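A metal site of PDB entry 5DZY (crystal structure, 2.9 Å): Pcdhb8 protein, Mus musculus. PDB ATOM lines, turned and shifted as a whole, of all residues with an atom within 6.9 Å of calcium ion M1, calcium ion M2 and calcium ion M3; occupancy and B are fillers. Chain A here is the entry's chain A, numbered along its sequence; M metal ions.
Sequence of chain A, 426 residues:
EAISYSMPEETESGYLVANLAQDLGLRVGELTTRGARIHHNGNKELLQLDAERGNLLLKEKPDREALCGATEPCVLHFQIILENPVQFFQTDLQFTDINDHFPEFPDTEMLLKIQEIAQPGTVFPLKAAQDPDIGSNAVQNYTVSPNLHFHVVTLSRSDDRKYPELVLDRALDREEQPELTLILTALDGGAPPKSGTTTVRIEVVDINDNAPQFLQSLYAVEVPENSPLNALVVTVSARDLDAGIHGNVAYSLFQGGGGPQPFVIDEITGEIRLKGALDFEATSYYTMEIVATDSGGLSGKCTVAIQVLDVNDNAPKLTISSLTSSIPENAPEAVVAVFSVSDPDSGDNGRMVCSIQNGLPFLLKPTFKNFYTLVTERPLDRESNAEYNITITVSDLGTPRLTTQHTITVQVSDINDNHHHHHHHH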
ATOM      1  N   GLU A 225       0.145  -6.549 -25.275  1.00  0.00           N
ATOM      2  CA  GLU A 225       0.535  -7.391 -26.402  1.00  0.00           C
ATOM      3  C   GLU A 225      -0.666  -8.131 -26.986  1.00  0.00           C
ATOM      4  O   GLU A 225      -0.757  -8.337 -28.196  1.00  0.00           O
ATOM      5  CB  GLU A 225       1.601  -8.387 -25.978  1.00  0.00           C
ATOM      6  CG  GLU A 225       2.035  -9.361 -27.065  1.00  0.00           C
ATOM      7  CD  GLU A 225       3.073 -10.357 -26.584  1.00  0.00           C
ATOM      8  OE1 GLU A 225       3.523 -10.233 -25.416  1.00  0.00           O
ATOM      9  OE2 GLU A 225       3.445 -11.251 -27.363  1.00  0.00           O
ATOM     10  N   LEU A 278       0.969  -7.729 -32.433  1.00  0.00           N
ATOM     11  CA  LEU A 278       1.994  -7.221 -31.533  1.00  0.00           C
ATOM     12  C   LEU A 278       2.617  -8.346 -30.709  1.00  0.00           C
ATOM     13  O   LEU A 278       1.931  -9.282 -30.311  1.00  0.00           O
ATOM     14  CB  LEU A 278       1.427  -6.155 -30.590  1.00  0.00           C
ATOM     15  CG  LEU A 278       1.378  -4.720 -31.129  1.00  0.00           C
ATOM     16  CD1 LEU A 278       0.832  -3.778 -30.071  1.00  0.00           C
ATOM     17  CD2 LEU A 278       2.760  -4.282 -31.586  1.00  0.00           C
ATOM     18  N   ASP A 279       3.925  -8.246 -30.491  1.00  0.00           N
ATOM     19  CA  ASP A 279       4.632  -9.235 -29.671  1.00  0.00           C
ATOM     20  C   ASP A 279       5.737  -8.561 -28.870  1.00  0.00           C
ATOM     21  O   ASP A 279       6.696  -8.029 -29.434  1.00  0.00           O
ATOM     22  CB  ASP A 279       5.217 -10.344 -30.551  1.00  0.00           C
ATOM     23  CG  ASP A 279       5.769 -11.492 -29.740  1.00  0.00           C
ATOM     24  OD1 ASP A 279       5.009 -12.439 -29.463  1.00  0.00           O
ATOM     25  OD2 ASP A 279       6.972 -11.453 -29.385  1.00  0.00           O
ATOM     26  N   PHE A 280       5.597  -8.597 -27.542  1.00  0.00           N
ATOM     27  CA  PHE A 280       6.552  -7.964 -26.648  1.00  0.00           C
ATOM     28  C   PHE A 280       7.939  -8.582 -26.756  1.00  0.00           C
ATOM     29  O   PHE A 280       8.946  -7.928 -26.498  1.00  0.00           O
ATOM     30  CB  PHE A 280       6.041  -8.049 -25.208  1.00  0.00           C
ATOM     31  CG  PHE A 280       6.943  -7.401 -24.197  1.00  0.00           C
ATOM     32  CD1 PHE A 280       6.883  -6.040 -23.958  1.00  0.00           C
ATOM     33  CD2 PHE A 280       7.860  -8.155 -23.473  1.00  0.00           C
ATOM     34  CE1 PHE A 280       7.711  -5.439 -23.029  1.00  0.00           C
ATOM     35  CE2 PHE A 280       8.693  -7.562 -22.541  1.00  0.00           C
ATOM     36  CZ  PHE A 280       8.614  -6.205 -22.317  1.00  0.00           C
ATOM     37  N   GLU A 281       7.982  -9.855 -27.152  1.00  0.00           N
ATOM     38  CA  GLU A 281       9.235 -10.587 -27.240  1.00  0.00           C
ATOM     39  C   GLU A 281       9.978 -10.266 -28.537  1.00  0.00           C
ATOM     40  O   GLU A 281      11.194 -10.450 -28.623  1.00  0.00           O
ATOM     41  CB  GLU A 281       8.987 -12.096 -27.138  1.00  0.00           C
ATOM     42  CG  GLU A 281       8.598 -12.571 -25.750  1.00  0.00           C
ATOM     43  CD  GLU A 281       7.242 -12.075 -25.309  1.00  0.00           C
ATOM     44  OE1 GLU A 281       6.331 -12.013 -26.163  1.00  0.00           O
ATOM     45  OE2 GLU A 281       7.081 -11.739 -24.117  1.00  0.00           O
ATOM     46  N   ALA A 282       9.252  -9.795 -29.543  1.00  0.00           N
ATOM     47  CA  ALA A 282       9.860  -9.399 -30.800  1.00  0.00           C
ATOM     48  C   ALA A 282      10.285  -7.930 -30.752  1.00  0.00           C
ATOM     49  O   ALA A 282      11.470  -7.619 -30.869  1.00  0.00           O
ATOM     50  CB  ALA A 282       8.899  -9.630 -31.956  1.00  0.00           C
ATOM     51  N   LEU A 309       3.087  -3.823 -23.634  1.00  0.00           N
ATOM     52  CA  LEU A 309       3.056  -4.510 -22.350  1.00  0.00           C
ATOM     53  C   LEU A 309       3.240  -6.011 -22.547  1.00  0.00           C
ATOM     54  O   LEU A 309       2.755  -6.584 -23.522  1.00  0.00           O
ATOM     55  CB  LEU A 309       1.753  -4.232 -21.617  1.00  0.00           C
ATOM     56  CG  LEU A 309       1.469  -2.773 -21.236  1.00  0.00           C
ATOM     57  CD1 LEU A 309       0.126  -2.663 -20.533  1.00  0.00           C
ATOM     58  CD2 LEU A 309       2.595  -2.224 -20.367  1.00  0.00           C
ATOM     59  N   ASP A 310       3.950  -6.649 -21.615  1.00  0.00           N
ATOM     60  CA  ASP A 310       4.214  -8.079 -21.699  1.00  0.00           C
ATOM     61  C   ASP A 310       3.002  -8.898 -21.245  1.00  0.00           C
ATOM     62  O   ASP A 310       2.372  -8.592 -20.233  1.00  0.00           O
ATOM     63  CB  ASP A 310       5.437  -8.454 -20.871  1.00  0.00           C
ATOM     64  CG  ASP A 310       5.739  -9.944 -20.914  1.00  0.00           C
ATOM     65  OD1 ASP A 310       5.482 -10.568 -21.962  1.00  0.00           O
ATOM     66  OD2 ASP A 310       6.238 -10.482 -19.904  1.00  0.00           O
ATOM     67  N   VAL A 311       2.691  -9.942 -22.002  1.00  0.00           N
ATOM     68  CA  VAL A 311       1.637 -10.876 -21.646  1.00  0.00           C
ATOM     69  C   VAL A 311       2.193 -12.298 -21.621  1.00  0.00           C
ATOM     70  O   VAL A 311       2.884 -12.708 -22.541  1.00  0.00           O
ATOM     71  CB  VAL A 311       0.444 -10.806 -22.621  1.00  0.00           C
ATOM     72  CG1 VAL A 311      -0.662 -11.765 -22.201  1.00  0.00           C
ATOM     73  CG2 VAL A 311      -0.087  -9.375 -22.706  1.00  0.00           C
ATOM     74  N   ASN A 312       1.889 -13.039 -20.558  1.00  0.00           N
ATOM     75  CA  ASN A 312       2.364 -14.409 -20.438  1.00  0.00           C
ATOM     76  C   ASN A 312       1.716 -15.319 -21.469  1.00  0.00           C
ATOM     77  O   ASN A 312       0.746 -16.026 -21.175  1.00  0.00           O
ATOM     78  CB  ASN A 312       2.110 -14.941 -19.031  1.00  0.00           C
ATOM     79  CG  ASN A 312       2.803 -16.267 -18.772  1.00  0.00           C
ATOM     80  OD1 ASN A 312       3.772 -16.615 -19.453  1.00  0.00           O
ATOM     81  ND2 ASN A 312       2.325 -17.001 -17.773  1.00  0.00           N
ATOM     82  N   ASP A 313       2.244 -15.303 -22.693  1.00  0.00           N
ATOM     83  CA  ASP A 313       1.688 -16.099 -23.776  1.00  0.00           C
ATOM     84  C   ASP A 313       2.710 -17.101 -24.318  1.00  0.00           C
ATOM     85  O   ASP A 313       2.538 -17.659 -25.404  1.00  0.00           O
ATOM     86  CB  ASP A 313       1.191 -15.194 -24.904  1.00  0.00           C
ATOM     87  CG  ASP A 313       2.301 -14.354 -25.523  1.00  0.00           C
ATOM     88  OD1 ASP A 313       3.353 -14.183 -24.869  1.00  0.00           O
ATOM     89  OD2 ASP A 313       2.113 -13.867 -26.656  1.00  0.00           O
ATOM     90  N   ASN A 314       3.787 -17.319 -23.557  1.00  0.00           N
ATOM     91  CA  ASN A 314       4.811 -18.273 -23.947  1.00  0.00           C
ATOM     92  C   ASN A 314       5.070 -19.333 -22.885  1.00  0.00           C
ATOM     93  O   ASN A 314       5.310 -19.010 -21.713  1.00  0.00           O
ATOM     94  CB  ASN A 314       6.121 -17.550 -24.280  1.00  0.00           C
ATOM     95  CG  ASN A 314       6.098 -16.898 -25.646  1.00  0.00           C
ATOM     96  OD1 ASN A 314       6.319 -15.696 -25.781  1.00  0.00           O
ATOM     97  ND2 ASN A 314       5.831 -17.692 -26.674  1.00  0.00           N
ATOM     98  N   ALA A 315       5.026 -20.591 -23.294  1.00  0.00           N
ATOM     99  CA  ALA A 315       5.339 -21.704 -22.398  1.00  0.00           C
ATOM    100  C   ALA A 315       6.842 -21.941 -22.365  1.00  0.00           C
ATOM    101  O   ALA A 315       7.531 -21.733 -23.365  1.00  0.00           O
ATOM    102  CB  ALA A 315       4.602 -22.963 -22.835  1.00  0.00           C
ATOM    103  N   PRO A 316       7.367 -22.367 -21.198  1.00  0.00           N
ATOM    104  CA  PRO A 316       8.799 -22.662 -21.053  1.00  0.00           C
ATOM    105  C   PRO A 316       9.286 -23.726 -22.029  1.00  0.00           C
ATOM    106  O   PRO A 316       8.606 -24.731 -22.228  1.00  0.00           O
ATOM    107  CB  PRO A 316       8.910 -23.162 -19.607  1.00  0.00           C
ATOM    108  CG  PRO A 316       7.737 -22.558 -18.907  1.00  0.00           C
ATOM    109  CD  PRO A 316       6.640 -22.518 -19.934  1.00  0.00           C
ATOM    110  N   SER A 342      14.158 -22.541 -21.236  1.00  0.00           N
ATOM    111  CA  SER A 342      14.130 -21.238 -21.889  1.00  0.00           C
ATOM    112  C   SER A 342      12.787 -20.544 -21.706  1.00  0.00           C
ATOM    113  O   SER A 342      11.766 -21.188 -21.497  1.00  0.00           O
ATOM    114  CB  SER A 342      14.456 -21.379 -23.376  1.00  0.00           C
ATOM    115  OG  SER A 342      14.426 -20.125 -24.028  1.00  0.00           O
ATOM    116  N   ASP A 343      12.795 -19.215 -21.788  1.00  0.00           N
ATOM    117  CA  ASP A 343      11.582 -18.418 -21.688  1.00  0.00           C
ATOM    118  C   ASP A 343      11.818 -17.013 -22.225  1.00  0.00           C
ATOM    119  O   ASP A 343      12.576 -16.243 -21.638  1.00  0.00           O
ATOM    120  CB  ASP A 343      11.087 -18.356 -20.234  1.00  0.00           C
ATOM    121  CG  ASP A 343       9.634 -17.948 -20.126  1.00  0.00           C
ATOM    122  OD1 ASP A 343       9.123 -17.267 -21.041  1.00  0.00           O
ATOM    123  OD2 ASP A 343       8.994 -18.304 -19.114  1.00  0.00           O
ATOM    124  N   PRO A 344      11.153 -16.670 -23.337  1.00  0.00           N
ATOM    125  CA  PRO A 344      11.309 -15.361 -23.985  1.00  0.00           C
ATOM    126  C   PRO A 344      10.604 -14.241 -23.223  1.00  0.00           C
ATOM    127  O   PRO A 344      10.890 -13.066 -23.459  1.00  0.00           O
ATOM    128  CB  PRO A 344      10.676 -15.573 -25.353  1.00  0.00           C
ATOM    129  CG  PRO A 344       9.653 -16.624 -25.123  1.00  0.00           C
ATOM    130  CD  PRO A 344      10.237 -17.540 -24.089  1.00  0.00           C
ATOM    131  N   ASP A 345       9.688 -14.598 -22.329  1.00  0.00           N
ATOM    132  CA  ASP A 345       8.939 -13.612 -21.555  1.00  0.00           C
ATOM    133  C   ASP A 345       9.830 -12.878 -20.561  1.00  0.00           C
ATOM    134  O   ASP A 345      10.993 -13.229 -20.369  1.00  0.00           O
ATOM    135  CB  ASP A 345       7.771 -14.282 -20.816  1.00  0.00           C
ATOM    136  CG  ASP A 345       6.781 -14.928 -21.762  1.00  0.00           C
ATOM    137  OD1 ASP A 345       6.641 -14.452 -22.906  1.00  0.00           O
ATOM    138  OD2 ASP A 345       6.137 -15.922 -21.359  1.00  0.00           O
ATOM    139  N   SER A 346       9.272 -11.842 -19.933  1.00  0.00           N
ATOM    140  CA  SER A 346      10.023 -11.045 -18.961  1.00  0.00           C
ATOM    141  C   SER A 346       9.374 -11.087 -17.579  1.00  0.00           C
ATOM    142  O   SER A 346       8.214 -11.463 -17.449  1.00  0.00           O
ATOM    143  CB  SER A 346      10.138  -9.600 -19.442  1.00  0.00           C
ATOM    144  OG  SER A 346       8.856  -9.003 -19.580  1.00  0.00           O
ATOM    145  N   ASP A 348       8.310 -12.245 -13.901  1.00  0.00           N
ATOM    146  CA  ASP A 348       7.931 -13.556 -13.366  1.00  0.00           C
ATOM    147  C   ASP A 348       7.404 -14.453 -14.478  1.00  0.00           C
ATOM    148  O   ASP A 348       7.381 -15.677 -14.339  1.00  0.00           O
ATOM    149  CB  ASP A 348       6.885 -13.398 -12.270  1.00  0.00           C
ATOM    150  CG  ASP A 348       7.420 -12.681 -11.045  1.00  0.00           C
ATOM    151  OD1 ASP A 348       8.660 -12.619 -10.890  1.00  0.00           O
ATOM    152  OD2 ASP A 348       6.613 -12.182 -10.237  1.00  0.00           O
ATOM    153  N   ASN A 349       6.982 -13.847 -15.583  1.00  0.00           N
ATOM    154  CA  ASN A 349       6.542 -14.597 -16.752  1.00  0.00           C
ATOM    155  C   ASN A 349       7.725 -15.302 -17.404  1.00  0.00           C
ATOM    156  O   ASN A 349       7.565 -16.321 -18.072  1.00  0.00           O
ATOM    157  CB  ASN A 349       5.857 -13.678 -17.765  1.00  0.00           C
ATOM    158  CG  ASN A 349       4.677 -12.939 -17.167  1.00  0.00           C
ATOM    159  OD1 ASN A 349       4.028 -13.413 -16.243  1.00  0.00           O
ATOM    160  ND2 ASN A 349       4.399 -11.755 -17.701  1.00  0.00           N
ATOM    161  N   GLY A 350       8.922 -14.753 -17.201  1.00  0.00           N
ATOM    162  CA  GLY A 350      10.138 -15.327 -17.732  1.00  0.00           C
ATOM    163  C   GLY A 350      10.844 -16.210 -16.720  1.00  0.00           C
ATOM    164  O   GLY A 350      11.561 -17.142 -17.090  1.00  0.00           O
ATOM    165  N   ARG A 351      10.633 -15.926 -15.438  1.00  0.00           N
ATOM    166  CA  ARG A 351      11.202 -16.729 -14.363  1.00  0.00           C
ATOM    167  C   ARG A 351      10.503 -18.079 -14.299  1.00  0.00           C
ATOM    168  O   ARG A 351       9.277 -18.144 -14.410  1.00  0.00           O
ATOM    169  CB  ARG A 351      11.106 -16.005 -13.027  1.00  0.00           C
ATOM    170  CG  ARG A 351      11.736 -16.758 -11.869  1.00  0.00           C
ATOM    171  CD  ARG A 351      11.775 -15.922 -10.600  1.00  0.00           C
ATOM    172  NE  ARG A 351      12.549 -14.694 -10.779  1.00  0.00           N
ATOM    173  CZ  ARG A 351      12.055 -13.475 -10.640  1.00  0.00           C
ATOM    174  NH1 ARG A 351      10.780 -13.313 -10.301  1.00  0.00           N
ATOM    175  NH2 ARG A 351      12.827 -12.407 -10.819  1.00  0.00           N
ATOM    176  N   ASP A 396       6.552 -21.714 -15.155  1.00  0.00           N
ATOM    177  CA  ASP A 396       6.865 -20.319 -14.881  1.00  0.00           C
ATOM    178  C   ASP A 396       6.161 -19.812 -13.619  1.00  0.00           C
ATOM    179  O   ASP A 396       5.265 -20.475 -13.091  1.00  0.00           O
ATOM    180  CB  ASP A 396       6.488 -19.432 -16.073  1.00  0.00           C
ATOM    181  CG  ASP A 396       5.088 -19.706 -16.595  1.00  0.00           C
ATOM    182  OD1 ASP A 396       4.214 -20.117 -15.804  1.00  0.00           O
ATOM    183  OD2 ASP A 396       4.861 -19.511 -17.812  1.00  0.00           O
ATOM    184  N   LEU A 397       6.561 -18.644 -13.153  1.00  0.00           N
ATOM    185  CA  LEU A 397       5.961 -18.046 -11.961  1.00  0.00           C
ATOM    186  C   LEU A 397       5.088 -16.849 -12.317  1.00  0.00           C
ATOM    187  O   LEU A 397       4.908 -15.935 -11.507  1.00  0.00           O
ATOM    188  CB  LEU A 397       7.057 -17.614 -10.976  1.00  0.00           C
ATOM    189  CG  LEU A 397       7.925 -18.732 -10.389  1.00  0.00           C
ATOM    190  CD1 LEU A 397       8.993 -18.154  -9.468  1.00  0.00           C
ATOM    191  CD2 LEU A 397       7.067 -19.747  -9.659  1.00  0.00           C
ATOM    192  N   GLY A 398       4.547 -16.862 -13.536  1.00  0.00           N
ATOM    193  CA  GLY A 398       3.718 -15.769 -14.006  1.00  0.00           C
ATOM    194  C   GLY A 398       2.236 -15.991 -13.754  1.00  0.00           C
ATOM    195  O   GLY A 398       1.843 -17.011 -13.187  1.00  0.00           O
ATOM    196  N   PRO A 400      -1.447 -15.804 -15.896  1.00  0.00           N
ATOM    197  CA  PRO A 400      -1.595 -17.177 -15.394  1.00  0.00           C
ATOM    198  C   PRO A 400      -0.329 -18.011 -15.563  1.00  0.00           C
ATOM    199  O   PRO A 400       0.563 -17.645 -16.336  1.00  0.00           O
ATOM    200  CB  PRO A 400      -2.729 -17.755 -16.257  1.00  0.00           C
ATOM    201  CG  PRO A 400      -3.392 -16.571 -16.887  1.00  0.00           C
ATOM    202  CD  PRO A 400      -2.303 -15.565 -17.080  1.00  0.00           C
ATOM    203  N   LEU A 402       1.996 -21.069 -16.728  1.00  0.00           N
ATOM    204  CA  LEU A 402       2.104 -22.016 -17.825  1.00  0.00           C
ATOM    205  C   LEU A 402       3.100 -23.132 -17.492  1.00  0.00           C
ATOM    206  O   LEU A 402       4.208 -22.873 -17.019  1.00  0.00           O
ATOM    207  CB  LEU A 402       2.534 -21.313 -19.109  1.00  0.00           C
ATOM    208  CG  LEU A 402       1.584 -20.248 -19.664  1.00  0.00           C
ATOM    209  CD1 LEU A 402       2.151 -19.622 -20.919  1.00  0.00           C
ATOM    210  CD2 LEU A 402       0.215 -20.852 -19.934  1.00  0.00           C
HETATM  211 CA    CA M   1       4.970 -12.423 -23.820  1.00  0.00          CA
HETATM  212 CA    CA M   2       4.417 -13.226 -27.170  1.00  0.00          CA
HETATM  213 CA    CA M   3       6.299 -17.723 -19.700  1.00  0.00          CA
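Six residues have an atom within 4 Å of calcium ion M3: Asn 312, Asn 314, Asp 343, Asp 345, Asn 349 and Asp 396.
The nearest printed residue that does not touch calcium ion M3 is Gly 350 (4.7 Å).
The side-chain carboxylate (OE2) of Glu 225 binds calcium ion M2 (2.2 Å).
Calcium ion M2 is bound by OD2 of Asp 313, at 2.4 Å.
The side-chain carboxylate (OE1) of Glu 281 binds calcium ion M2 (2.5 Å).
The side-chain carboxylate (OD1) of Asp 279 is bound to calcium ion M2, 2.5 Å away.
Calcium ion M2 is bound by the side-chain carboxylate (OD1) of Asp 313 (2.7 Å).
Calcium ion M2 has five donor atoms within binding distance.
Within 4 Å of calcium ion M1: Glu 225, Glu 281, Asp 310, Val 311, Asp 313 and Asp 345.
The nearest printed residue that does not touch calcium ion M1 is Asn 314 (4.05 Å).
Calcium ion M3 is bound by the side-chain carboxylate (OD2) of Asp 345, 2.5 Å away.
O of Asn 349 binds calcium ion M3 (2.5 Å).
O of Asn 314 is bound to calcium ion M3 (2.6 Å).
Calcium ion M3 is bound by OD1 of Asn 312 (2.8 Å).
Calcium ion M3 is bound by OD2 of Asp 343 (2.8 Å).
Calcium ion M3 has five donor atoms within binding distance.
Slightly farther from calcium ion M3 lies OD2 of Asp 396 (3.0 Å).
The backbone NH of Phe 280 lies close to the side-chain carboxylate of Glu 225 (3.4 Å).
N of Glu 225 sits at hydrogen-bond distance from O of Leu 309, at 3.1 Å.
OD1 of Asp 313 sits close to OD1 of Asn 314, at 3.5 Å.
The side-chain amide nitrogen (ND2) of Asn 349 is in hydrogen-bond range of the side-chain carboxylate (OD2) of Asp 310.
The backbone NH (N) of Ala 282 sits at hydrogen-bond distance from the side-chain carboxylate (OD2) of Asp 279 (2.8 Å).
The side-chain hydroxyl of Ser 346 lies within hydrogen-bond range of the side-chain carboxylate of Asp 310 (3.0 Å).
The side-chain carboxylate of Asp 396 lies within hydrogen-bond range of the backbone NH of Leu 402 (2.6 Å).
The nearest printed residue that does not touch calcium ion M2 is Phe 280 (4.8 Å).
Calcium ion M1 is bound by OE2 of Glu 281 (2.2 Å), O of Val 311 (2.5 Å), OD1 of Asp 313 (2.6 Å), OD1 of Asp 310 (2.7 Å), OE1 of Glu 281 (2.7 Å) and OD1 of Asp 345 (2.8 Å).
Slightly farther from calcium ion M1 lies the side-chain carboxylate (OE1) of Glu 225 (3.1 Å).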
